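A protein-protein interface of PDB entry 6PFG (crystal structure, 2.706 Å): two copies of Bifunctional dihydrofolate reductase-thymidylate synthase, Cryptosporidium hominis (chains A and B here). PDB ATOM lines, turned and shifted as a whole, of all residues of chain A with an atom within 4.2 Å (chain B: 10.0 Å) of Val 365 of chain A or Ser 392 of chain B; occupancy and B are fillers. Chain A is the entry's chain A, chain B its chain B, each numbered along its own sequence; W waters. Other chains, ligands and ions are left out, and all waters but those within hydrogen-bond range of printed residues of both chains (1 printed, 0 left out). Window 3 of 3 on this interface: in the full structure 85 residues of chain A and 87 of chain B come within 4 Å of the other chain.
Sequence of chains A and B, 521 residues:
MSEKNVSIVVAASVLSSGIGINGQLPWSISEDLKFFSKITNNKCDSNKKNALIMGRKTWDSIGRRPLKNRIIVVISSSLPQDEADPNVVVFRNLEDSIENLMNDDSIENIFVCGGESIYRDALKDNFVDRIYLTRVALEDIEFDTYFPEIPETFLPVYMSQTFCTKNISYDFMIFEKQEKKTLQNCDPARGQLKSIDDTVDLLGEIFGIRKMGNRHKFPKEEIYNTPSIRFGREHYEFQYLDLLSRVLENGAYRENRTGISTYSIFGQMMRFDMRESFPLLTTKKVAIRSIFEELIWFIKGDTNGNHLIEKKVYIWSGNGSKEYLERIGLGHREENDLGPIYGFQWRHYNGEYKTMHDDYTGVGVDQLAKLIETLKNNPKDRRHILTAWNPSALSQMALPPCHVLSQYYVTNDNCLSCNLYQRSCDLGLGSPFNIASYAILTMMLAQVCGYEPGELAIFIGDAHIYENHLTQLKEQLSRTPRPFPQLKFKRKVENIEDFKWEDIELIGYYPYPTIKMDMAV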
ATOM      1  N   TRP A 346      28.434 -19.968  -0.837  1.00  0.00           N
ATOM      2  CA  TRP A 346      28.686 -20.375  -2.216  1.00  0.00           C
ATOM      3  C   TRP A 346      27.386 -20.623  -2.967  1.00  0.00           C
ATOM      4  O   TRP A 346      27.249 -20.226  -4.130  1.00  0.00           O
ATOM      5  CB  TRP A 346      29.551 -21.635  -2.252  1.00  0.00           C
ATOM      6  CG  TRP A 346      30.980 -21.438  -1.853  1.00  0.00           C
ATOM      7  CD1 TRP A 346      31.513 -20.373  -1.189  1.00  0.00           C
ATOM      8  CD2 TRP A 346      32.064 -22.340  -2.101  1.00  0.00           C
ATOM      9  NE1 TRP A 346      32.863 -20.557  -1.004  1.00  0.00           N
ATOM     10  CE2 TRP A 346      33.226 -21.757  -1.556  1.00  0.00           C
ATOM     11  CE3 TRP A 346      32.165 -23.585  -2.731  1.00  0.00           C
ATOM     12  CZ2 TRP A 346      34.471 -22.376  -1.623  1.00  0.00           C
ATOM     13  CZ3 TRP A 346      33.402 -24.197  -2.796  1.00  0.00           C
ATOM     14  CH2 TRP A 346      34.539 -23.593  -2.246  1.00  0.00           C
ATOM     15  N   ARG A 347      26.423 -21.288  -2.325  1.00  0.00           N
ATOM     16  CA  ARG A 347      25.199 -21.702  -2.994  1.00  0.00           C
ATOM     17  C   ARG A 347      23.973 -20.899  -2.591  1.00  0.00           C
ATOM     18  O   ARG A 347      23.019 -20.834  -3.372  1.00  0.00           O
ATOM     19  CB  ARG A 347      24.920 -23.189  -2.725  1.00  0.00           C
ATOM     20  CG  ARG A 347      26.117 -24.100  -2.945  1.00  0.00           C
ATOM     21  CD  ARG A 347      26.714 -23.920  -4.331  1.00  0.00           C
ATOM     22  NE  ARG A 347      25.715 -24.076  -5.382  1.00  0.00           N
ATOM     23  CZ  ARG A 347      25.349 -25.246  -5.895  1.00  0.00           C
ATOM     24  NH1 ARG A 347      25.900 -26.369  -5.451  1.00  0.00           N
ATOM     25  NH2 ARG A 347      24.429 -25.294  -6.850  1.00  0.00           N
ATOM     26  N   HIS A 348      23.967 -20.294  -1.402  1.00  0.00           N
ATOM     27  CA  HIS A 348      22.813 -19.554  -0.902  1.00  0.00           C
ATOM     28  C   HIS A 348      23.282 -18.269  -0.215  1.00  0.00           C
ATOM     29  O   HIS A 348      23.059 -18.047   0.971  1.00  0.00           O
ATOM     30  CB  HIS A 348      21.986 -20.409   0.059  1.00  0.00           C
ATOM     31  CG  HIS A 348      21.758 -21.811  -0.413  1.00  0.00           C
ATOM     32  ND1 HIS A 348      20.862 -22.126  -1.413  1.00  0.00           N
ATOM     33  CD2 HIS A 348      22.305 -22.985  -0.016  1.00  0.00           C
ATOM     34  CE1 HIS A 348      20.868 -23.433  -1.612  1.00  0.00           C
ATOM     35  NE2 HIS A 348      21.734 -23.978  -0.776  1.00  0.00           N
ATOM     36  N   TYR A 349      23.960 -17.407  -0.969  1.00  0.00           N
ATOM     37  CA  TYR A 349      24.486 -16.176  -0.392  1.00  0.00           C
ATOM     38  C   TYR A 349      23.347 -15.269   0.055  1.00  0.00           C
ATOM     39  O   TYR A 349      22.350 -15.103  -0.652  1.00  0.00           O
ATOM     40  CB  TYR A 349      25.372 -15.446  -1.401  1.00  0.00           C
ATOM     41  CG  TYR A 349      26.129 -14.286  -0.796  1.00  0.00           C
ATOM     42  CD1 TYR A 349      27.364 -14.481  -0.192  1.00  0.00           C
ATOM     43  CD2 TYR A 349      25.608 -12.999  -0.823  1.00  0.00           C
ATOM     44  CE1 TYR A 349      28.059 -13.427   0.366  1.00  0.00           C
ATOM     45  CE2 TYR A 349      26.294 -11.939  -0.265  1.00  0.00           C
ATOM     46  CZ  TYR A 349      27.522 -12.158   0.326  1.00  0.00           C
ATOM     47  OH  TYR A 349      28.214 -11.108   0.883  1.00  0.00           O
ATOM     48  N   ASN A 350      23.503 -14.679   1.244  1.00  0.00           N
ATOM     49  CA  ASN A 350      22.488 -13.836   1.878  1.00  0.00           C
ATOM     50  C   ASN A 350      21.208 -14.602   2.187  1.00  0.00           C
ATOM     51  O   ASN A 350      20.144 -13.996   2.347  1.00  0.00           O
ATOM     52  CB  ASN A 350      22.161 -12.598   1.033  1.00  0.00           C
ATOM     53  CG  ASN A 350      23.148 -11.473   1.242  1.00  0.00           C
ATOM     54  OD1 ASN A 350      23.744 -11.346   2.312  1.00  0.00           O
ATOM     55  ND2 ASN A 350      23.316 -10.637   0.225  1.00  0.00           N
ATOM     56  N   GLY A 364      18.656 -17.382  -1.513  1.00  0.00           N
ATOM     57  CA  GLY A 364      19.994 -16.857  -1.671  1.00  0.00           C
ATOM     58  C   GLY A 364      20.494 -16.910  -3.103  1.00  0.00           C
ATOM     59  O   GLY A 364      19.862 -17.457  -4.008  1.00  0.00           O
ATOM     60  N   VAL A 365      21.669 -16.319  -3.302  1.00  0.00           N
ATOM     61  CA  VAL A 365      22.310 -16.271  -4.611  1.00  0.00           C
ATOM     62  C   VAL A 365      23.225 -17.478  -4.753  1.00  0.00           C
ATOM     63  O   VAL A 365      24.089 -17.719  -3.901  1.00  0.00           O
ATOM     64  CB  VAL A 365      23.095 -14.962  -4.792  1.00  0.00           C
ATOM     65  CG1 VAL A 365      23.760 -14.924  -6.157  1.00  0.00           C
ATOM     66  CG2 VAL A 365      22.179 -13.761  -4.610  1.00  0.00           C
ATOM     67  N   ASP A 366      23.040 -18.240  -5.832  1.00  0.00           N
ATOM     68  CA  ASP A 366      23.885 -19.399  -6.115  1.00  0.00           C
ATOM     69  C   ASP A 366      25.110 -18.897  -6.865  1.00  0.00           C
ATOM     70  O   ASP A 366      25.113 -18.785  -8.092  1.00  0.00           O
ATOM     71  CB  ASP A 366      23.124 -20.451  -6.911  1.00  0.00           C
ATOM     72  CG  ASP A 366      23.825 -21.801  -6.915  1.00  0.00           C
ATOM     73  OD1 ASP A 366      25.058 -21.842  -6.714  1.00  0.00           O
ATOM     74  OD2 ASP A 366      23.143 -22.826  -7.129  1.00  0.00           O
ATOM     75  N   GLN A 367      26.171 -18.590  -6.114  1.00  0.00           N
ATOM     76  CA  GLN A 367      27.375 -18.046  -6.731  1.00  0.00           C
ATOM     77  C   GLN A 367      28.046 -19.064  -7.641  1.00  0.00           C
ATOM     78  O   GLN A 367      28.564 -18.704  -8.703  1.00  0.00           O
ATOM     79  CB  GLN A 367      28.356 -17.577  -5.659  1.00  0.00           C
ATOM     80  CG  GLN A 367      27.949 -16.325  -4.913  1.00  0.00           C
ATOM     81  CD  GLN A 367      29.083 -15.776  -4.076  1.00  0.00           C
ATOM     82  OE1 GLN A 367      29.924 -15.023  -4.567  1.00  0.00           O
ATOM     83  NE2 GLN A 367      29.126 -16.167  -2.808  1.00  0.00           N
ATOM     84  N   LYS A 370      26.121 -19.443 -11.124  1.00  0.00           N
ATOM     85  CA  LYS A 370      26.346 -18.264 -11.953  1.00  0.00           C
ATOM     86  C   LYS A 370      27.798 -18.187 -12.407  1.00  0.00           C
ATOM     87  O   LYS A 370      28.083 -17.768 -13.535  1.00  0.00           O
ATOM     88  CB  LYS A 370      25.940 -17.002 -11.190  1.00  0.00           C
ATOM     89  CG  LYS A 370      24.517 -17.057 -10.644  1.00  0.00           C
ATOM     90  CD  LYS A 370      24.095 -15.755  -9.974  1.00  0.00           C
ATOM     91  CE  LYS A 370      23.637 -14.730 -10.997  1.00  0.00           C
ATOM     92  NZ  LYS A 370      23.063 -13.519 -10.349  1.00  0.00           N
ATOM     93  N   ARG B 333      17.287   4.674 -13.822  1.00  0.00           N
ATOM     94  CA  ARG B 333      18.105   5.368 -12.842  1.00  0.00           C
ATOM     95  C   ARG B 333      18.287   6.834 -13.222  1.00  0.00           C
ATOM     96  O   ARG B 333      18.301   7.198 -14.400  1.00  0.00           O
ATOM     97  CB  ARG B 333      19.463   4.673 -12.738  1.00  0.00           C
ATOM     98  CG  ARG B 333      20.223   4.921 -11.462  1.00  0.00           C
ATOM     99  CD  ARG B 333      19.520   4.350 -10.239  1.00  0.00           C
ATOM    100  NE  ARG B 333      19.388   2.896 -10.280  1.00  0.00           N
ATOM    101  CZ  ARG B 333      20.369   2.044 -10.003  1.00  0.00           C
ATOM    102  NH1 ARG B 333      21.573   2.495  -9.680  1.00  0.00           N
ATOM    103  NH2 ARG B 333      20.152   0.737 -10.060  1.00  0.00           N
ATOM    104  N   PRO B 340      24.252   1.088  -5.497  1.00  0.00           N
ATOM    105  CA  PRO B 340      24.990   0.670  -4.297  1.00  0.00           C
ATOM    106  C   PRO B 340      26.400   0.202  -4.612  1.00  0.00           C
ATOM    107  O   PRO B 340      26.618  -0.989  -4.856  1.00  0.00           O
ATOM    108  CB  PRO B 340      24.134  -0.479  -3.751  1.00  0.00           C
ATOM    109  CG  PRO B 340      23.470  -1.051  -4.970  1.00  0.00           C
ATOM    110  CD  PRO B 340      23.229   0.106  -5.902  1.00  0.00           C
ATOM    111  N   PHE B 344      28.651   2.400  -0.304  1.00  0.00           N
ATOM    112  CA  PHE B 344      27.360   1.927   0.165  1.00  0.00           C
ATOM    113  C   PHE B 344      27.459   0.536   0.755  1.00  0.00           C
ATOM    114  O   PHE B 344      26.730   0.221   1.698  1.00  0.00           O
ATOM    115  CB  PHE B 344      26.327   1.927  -0.967  1.00  0.00           C
ATOM    116  CG  PHE B 344      24.923   1.658  -0.499  1.00  0.00           C
ATOM    117  CD1 PHE B 344      24.104   2.701  -0.097  1.00  0.00           C
ATOM    118  CD2 PHE B 344      24.428   0.364  -0.442  1.00  0.00           C
ATOM    119  CE1 PHE B 344      22.813   2.461   0.343  1.00  0.00           C
ATOM    120  CE2 PHE B 344      23.138   0.117  -0.002  1.00  0.00           C
ATOM    121  CZ  PHE B 344      22.329   1.166   0.392  1.00  0.00           C
ATOM    122  N   GLN B 345      28.366  -0.290   0.238  1.00  0.00           N
ATOM    123  CA  GLN B 345      28.727  -1.521   0.922  1.00  0.00           C
ATOM    124  C   GLN B 345      29.652  -1.261   2.102  1.00  0.00           C
ATOM    125  O   GLN B 345      29.700  -2.078   3.028  1.00  0.00           O
ATOM    126  CB  GLN B 345      29.385  -2.492  -0.060  1.00  0.00           C
ATOM    127  CG  GLN B 345      28.628  -2.646  -1.368  1.00  0.00           C
ATOM    128  CD  GLN B 345      27.211  -3.155  -1.177  1.00  0.00           C
ATOM    129  OE1 GLN B 345      26.940  -3.955  -0.282  1.00  0.00           O
ATOM    130  NE2 GLN B 345      26.297  -2.684  -2.017  1.00  0.00           N
ATOM    131  N   TYR B 349      26.099  -2.152   4.188  1.00  0.00           N
ATOM    132  CA  TYR B 349      26.207  -3.417   3.474  1.00  0.00           C
ATOM    133  C   TYR B 349      24.910  -4.210   3.575  1.00  0.00           C
ATOM    134  O   TYR B 349      24.297  -4.296   4.642  1.00  0.00           O
ATOM    135  CB  TYR B 349      27.368  -4.247   4.019  1.00  0.00           C
ATOM    136  CG  TYR B 349      27.681  -5.455   3.168  1.00  0.00           C
ATOM    137  CD1 TYR B 349      28.551  -5.358   2.091  1.00  0.00           C
ATOM    138  CD2 TYR B 349      27.098  -6.688   3.432  1.00  0.00           C
ATOM    139  CE1 TYR B 349      28.838  -6.455   1.303  1.00  0.00           C
ATOM    140  CE2 TYR B 349      27.377  -7.790   2.649  1.00  0.00           C
ATOM    141  CZ  TYR B 349      28.249  -7.669   1.587  1.00  0.00           C
ATOM    142  OH  TYR B 349      28.532  -8.764   0.803  1.00  0.00           O
ATOM    143  N   ASN B 350      24.499  -4.794   2.446  1.00  0.00           N
ATOM    144  CA  ASN B 350      23.250  -5.546   2.312  1.00  0.00           C
ATOM    145  C   ASN B 350      22.019  -4.678   2.543  1.00  0.00           C
ATOM    146  O   ASN B 350      20.936  -5.199   2.823  1.00  0.00           O
ATOM    147  CB  ASN B 350      23.214  -6.758   3.252  1.00  0.00           C
ATOM    148  CG  ASN B 350      23.964  -7.951   2.697  1.00  0.00           C
ATOM    149  OD1 ASN B 350      24.070  -8.120   1.483  1.00  0.00           O
ATOM    150  ND2 ASN B 350      24.486  -8.788   3.586  1.00  0.00           N
ATOM    151  N   GLY B 351      22.154  -3.361   2.416  1.00  0.00           N
ATOM    152  CA  GLY B 351      21.014  -2.481   2.600  1.00  0.00           C
ATOM    153  C   GLY B 351      20.182  -2.382   1.331  1.00  0.00           C
ATOM    154  O   GLY B 351      20.706  -2.324   0.220  1.00  0.00           O
ATOM    155  N   GLU B 352      18.864  -2.372   1.511  1.00  0.00           N
ATOM    156  CA  GLU B 352      17.947  -2.262   0.382  1.00  0.00           C
ATOM    157  C   GLU B 352      18.088  -0.880  -0.244  1.00  0.00           C
ATOM    158  O   GLU B 352      17.670   0.123   0.342  1.00  0.00           O
ATOM    159  CB  GLU B 352      16.512  -2.518   0.832  1.00  0.00           C
ATOM    160  CG  GLU B 352      15.531  -2.654  -0.317  1.00  0.00           C
ATOM    161  CD  GLU B 352      15.892  -3.791  -1.253  1.00  0.00           C
ATOM    162  OE1 GLU B 352      16.312  -4.858  -0.757  1.00  0.00           O
ATOM    163  OE2 GLU B 352      15.766  -3.615  -2.485  1.00  0.00           O
ATOM    164  N   TYR B 353      18.683  -0.827  -1.432  1.00  0.00           N
ATOM    165  CA  TYR B 353      18.932   0.437  -2.106  1.00  0.00           C
ATOM    166  C   TYR B 353      17.705   0.873  -2.896  1.00  0.00           C
ATOM    167  O   TYR B 353      17.034   0.054  -3.532  1.00  0.00           O
ATOM    168  CB  TYR B 353      20.143   0.308  -3.033  1.00  0.00           C
ATOM    169  CG  TYR B 353      20.665   1.617  -3.586  1.00  0.00           C
ATOM    170  CD1 TYR B 353      21.565   2.387  -2.859  1.00  0.00           C
ATOM    171  CD2 TYR B 353      20.272   2.076  -4.838  1.00  0.00           C
ATOM    172  CE1 TYR B 353      22.054   3.581  -3.356  1.00  0.00           C
ATOM    173  CE2 TYR B 353      20.755   3.272  -5.345  1.00  0.00           C
ATOM    174  CZ  TYR B 353      21.648   4.020  -4.598  1.00  0.00           C
ATOM    175  OH  TYR B 353      22.136   5.209  -5.091  1.00  0.00           O
ATOM    176  N   ALA B 388      33.508  -5.044  -0.588  1.00  0.00           N
ATOM    177  CA  ALA B 388      32.510  -4.378  -1.407  1.00  0.00           C
ATOM    178  C   ALA B 388      31.813  -5.329  -2.366  1.00  0.00           C
ATOM    179  O   ALA B 388      30.896  -4.904  -3.079  1.00  0.00           O
ATOM    180  CB  ALA B 388      33.144  -3.226  -2.199  1.00  0.00           C
ATOM    181  N   TRP B 389      32.210  -6.598  -2.405  1.00  0.00           N
ATOM    182  CA  TRP B 389      31.639  -7.551  -3.353  1.00  0.00           C
ATOM    183  C   TRP B 389      30.369  -8.131  -2.746  1.00  0.00           C
ATOM    184  O   TRP B 389      30.420  -9.042  -1.915  1.00  0.00           O
ATOM    185  CB  TRP B 389      32.641  -8.645  -3.704  1.00  0.00           C
ATOM    186  CG  TRP B 389      32.215  -9.410  -4.906  1.00  0.00           C
ATOM    187  CD1 TRP B 389      31.634 -10.643  -4.933  1.00  0.00           C
ATOM    188  CD2 TRP B 389      32.301  -8.975  -6.267  1.00  0.00           C
ATOM    189  NE1 TRP B 389      31.365 -11.010  -6.231  1.00  0.00           N
ATOM    190  CE2 TRP B 389      31.765 -10.002  -7.069  1.00  0.00           C
ATOM    191  CE3 TRP B 389      32.787  -7.820  -6.887  1.00  0.00           C
ATOM    192  CZ2 TRP B 389      31.703  -9.909  -8.457  1.00  0.00           C
ATOM    193  CZ3 TRP B 389      32.722  -7.728  -8.266  1.00  0.00           C
ATOM    194  CH2 TRP B 389      32.184  -8.766  -9.034  1.00  0.00           C
ATOM    195  N   ASN B 390      29.224  -7.615  -3.180  1.00  0.00           N
ATOM    196  CA  ASN B 390      27.918  -8.071  -2.702  1.00  0.00           C
ATOM    197  C   ASN B 390      27.155  -8.672  -3.871  1.00  0.00           C
ATOM    198  O   ASN B 390      26.594  -7.929  -4.697  1.00  0.00           O
ATOM    199  CB  ASN B 390      27.136  -6.915  -2.083  1.00  0.00           C
ATOM    200  CG  ASN B 390      25.942  -7.381  -1.274  1.00  0.00           C
ATOM    201  OD1 ASN B 390      25.389  -8.455  -1.516  1.00  0.00           O
ATOM    202  ND2 ASN B 390      25.538  -6.571  -0.304  1.00  0.00           N
ATOM    203  N   PRO B 391      27.104 -10.003  -3.987  1.00  0.00           N
ATOM    204  CA  PRO B 391      26.396 -10.618  -5.124  1.00  0.00           C
ATOM    205  C   PRO B 391      24.939 -10.209  -5.239  1.00  0.00           C
ATOM    206  O   PRO B 391      24.384 -10.232  -6.346  1.00  0.00           O
ATOM    207  CB  PRO B 391      26.535 -12.122  -4.845  1.00  0.00           C
ATOM    208  CG  PRO B 391      27.776 -12.237  -4.023  1.00  0.00           C
ATOM    209  CD  PRO B 391      27.818 -10.998  -3.169  1.00  0.00           C
ATOM    210  N   SER B 392      24.295  -9.830  -4.132  1.00  0.00           N
ATOM    211  CA  SER B 392      22.890  -9.444  -4.187  1.00  0.00           C
ATOM    212  C   SER B 392      22.679  -8.091  -4.853  1.00  0.00           C
ATOM    213  O   SER B 392      21.577  -7.824  -5.342  1.00  0.00           O
ATOM    214  CB  SER B 392      22.296  -9.417  -2.779  1.00  0.00           C
ATOM    215  OG  SER B 392      22.407 -10.682  -2.148  1.00  0.00           O
ATOM    216  N   ALA B 393      23.706  -7.244  -4.905  1.00  0.00           N
ATOM    217  CA  ALA B 393      23.563  -5.885  -5.406  1.00  0.00           C
ATOM    218  C   ALA B 393      24.348  -5.616  -6.683  1.00  0.00           C
ATOM    219  O   ALA B 393      24.322  -4.484  -7.175  1.00  0.00           O
ATOM    220  CB  ALA B 393      23.986  -4.882  -4.327  1.00  0.00           C
ATOM    221  N   LEU B 394      25.033  -6.621  -7.237  1.00  0.00           N
ATOM    222  CA  LEU B 394      25.868  -6.390  -8.412  1.00  0.00           C
ATOM    223  C   LEU B 394      25.051  -5.846  -9.579  1.00  0.00           C
ATOM    224  O   LEU B 394      25.513  -4.965 -10.312  1.00  0.00           O
ATOM    225  CB  LEU B 394      26.573  -7.686  -8.816  1.00  0.00           C
ATOM    226  CG  LEU B 394      27.570  -8.265  -7.810  1.00  0.00           C
ATOM    227  CD1 LEU B 394      28.140  -9.578  -8.318  1.00  0.00           C
ATOM    228  CD2 LEU B 394      28.684  -7.269  -7.515  1.00  0.00           C
ATOM    229  N   SER B 395      23.827  -6.350  -9.758  1.00  0.00           N
ATOM    230  CA  SER B 395      23.006  -5.922 -10.886  1.00  0.00           C
ATOM    231  C   SER B 395      22.578  -4.464 -10.761  1.00  0.00           C
ATOM    232  O   SER B 395      22.359  -3.798 -11.779  1.00  0.00           O
ATOM    233  CB  SER B 395      21.778  -6.823 -11.012  1.00  0.00           C
ATOM    234  OG  SER B 395      21.023  -6.820  -9.812  1.00  0.00           O
ATOM    235  N   GLN B 396      22.455  -3.952  -9.534  1.00  0.00           N
ATOM    236  CA  GLN B 396      22.047  -2.569  -9.321  1.00  0.00           C
ATOM    237  C   GLN B 396      23.192  -1.575  -9.454  1.00  0.00           C
ATOM    238  O   GLN B 396      22.938  -0.366  -9.470  1.00  0.00           O
ATOM    239  CB  GLN B 396      21.415  -2.405  -7.937  1.00  0.00           C
ATOM    240  CG  GLN B 396      20.175  -3.241  -7.691  1.00  0.00           C
ATOM    241  CD  GLN B 396      19.584  -2.993  -6.315  1.00  0.00           C
ATOM    242  OE1 GLN B 396      19.727  -3.814  -5.409  1.00  0.00           O
ATOM    243  NE2 GLN B 396      18.924  -1.852  -6.149  1.00  0.00           N
ATOM    244  N   MET B 397      24.433  -2.043  -9.554  1.00  0.00           N
ATOM    245  CA  MET B 397      25.574  -1.140  -9.586  1.00  0.00           C
ATOM    246  C   MET B 397      25.827  -0.636 -10.999  1.00  0.00           C
ATOM    247  O   MET B 397      25.671  -1.371 -11.977  1.00  0.00           O
ATOM    248  CB  MET B 397      26.831  -1.835  -9.057  1.00  0.00           C
ATOM    249  CG  MET B 397      26.685  -2.427  -7.669  1.00  0.00           C
ATOM    250  SD  MET B 397      28.252  -3.006  -6.990  1.00  0.00           S
ATOM    251  CE  MET B 397      27.696  -3.930  -5.558  1.00  0.00           C
ATOM    252  N   PRO B 401      32.442  -3.695  -8.244  1.00  0.00           N
ATOM    253  CA  PRO B 401      33.638  -3.184  -7.559  1.00  0.00           C
ATOM    254  C   PRO B 401      34.921  -3.736  -8.164  1.00  0.00           C
ATOM    255  O   PRO B 401      35.043  -4.939  -8.408  1.00  0.00           O
ATOM    256  CB  PRO B 401      33.451  -3.662  -6.114  1.00  0.00           C
ATOM    257  CG  PRO B 401      31.997  -3.991  -5.993  1.00  0.00           C
ATOM    258  CD  PRO B 401      31.577  -4.471  -7.342  1.00  0.00           C
HETATM  259  O   HOH W   1      29.923 -13.656  -6.614  1.00  0.00           O
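OD1 of Asn 350 of chain B lies within hydrogen-bond range of ND2 of Asn 350 of chain A, 2.9 Å away. The side-chain amide nitrogen (ND2) of Asn 350 of chain A sits at hydrogen-bond distance from the side-chain amide oxygen (OD1) of Asn 390 of chain B (3.5 Å). The side-chain amide nitrogen (ND2) of Asn 350 of chain A lies within hydrogen-bond range of the side-chain hydroxyl (OG) of Ser 392 of chain B (2.5 Å). The side-chain hydroxyl of Tyr 349 of chain B sits close to the side-chain hydroxyl of Tyr 349 of chain A (2.4 Å).
N of Gln 367 of chain A lies within hydrogen-bond range of O of Trp 346 of chain A (2.8 Å). The backbone NH (N) of Tyr 349 of chain A is in hydrogen-bond range of the backbone carbonyl oxygen (O) of Val 365 of chain A, 3.0 Å away. O of Phe 344 of chain B sits at hydrogen-bond distance from N of Tyr 349 of chain B. The side-chain amide nitrogen of Asn 390 of chain B sits at hydrogen-bond distance from the side-chain amide oxygen of Gln 345 of chain B, at 3.0 Å. The side-chain amide oxygen (OD1) of Asn 350 of chain B is in hydrogen-bond range of the side-chain amide nitrogen (ND2) of Asn 390 of chain B. The side-chain amide oxygen (OD1) of Asn 390 of chain B sits close to the backbone NH (N) of Ser 392 of chain B.
Among the printed residues, merely in contact across the chains: Tyr 349 of chain A with Asn 390 of chain B, Tyr 349 of chain A with Pro 391 of chain B, Val 365 of chain A with Ser 392 of chain B and Gln 367 of chain A with Pro 391 of chain B.
Val 365 of chain A touches one residue of chain B. Ser 392 of chain B touches just these residues of chain A: Asn 350 (2.5 Å) and Val 365 (3.9 Å). No residue of chain B comes within 4 Å of Gly 364 of chain A. Asp 366 of chain A touches none of the printed residues of chain B. Printed residues of chain A within 4 Å of Pro 391 of chain B: Tyr 349 and Gln 367. Of the printed residues of chain A, Asn 350 of chain B touches Asn 350 (2.9 Å). Of the printed residues of chain B, Gln 367 of chain A touches Pro 391. Of the printed residues of chain A, Tyr 349 of chain B touches Tyr 349 (2.4 Å). Printed residues of chain B within 4 Å of Asn 350 of chain A: Asn 350, Asn 390 and Ser 392. Ala 393 of chain B touches none of the printed residues of chain A. His 348 of chain A touches none of the printed residues of chain B. The nearest residue of chain B that does not touch Val 365 of chain A is Pro 391 of chain B (4.2 Å).
Printed residues of chain A that touch a printed residue of chain B: Tyr 349, Asn 350, Val 365 and Gln 367. Hydrophobic or aromatic side chains of chain B that line the printed part of chain A: Tyr 349 and Pro 391. Among the printed residues, 8 pairs touch across the chains. Among the printed residues, no Asp or Glu carboxylate lies within 4 Å of a Lys or Arg side-chain nitrogen of the other chain.
Tyr 349 of chain A touches its own counterpart, Tyr 349 of chain B. Asn 350 of chain B touches its own counterpart, Asn 350 of chain A. Positions printed for both chains: 349 and 350. Of the 8 pairs that touch across the chains among the printed residues, 2 have their exchanged pair printed and touching as well.
Water W1 bridges the side-chain amide oxygen (OE1) of Gln 367 of chain A (2.5 Å) and the indole nitrogen (NE1) of Trp 389 of chain B (3.0 Å).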
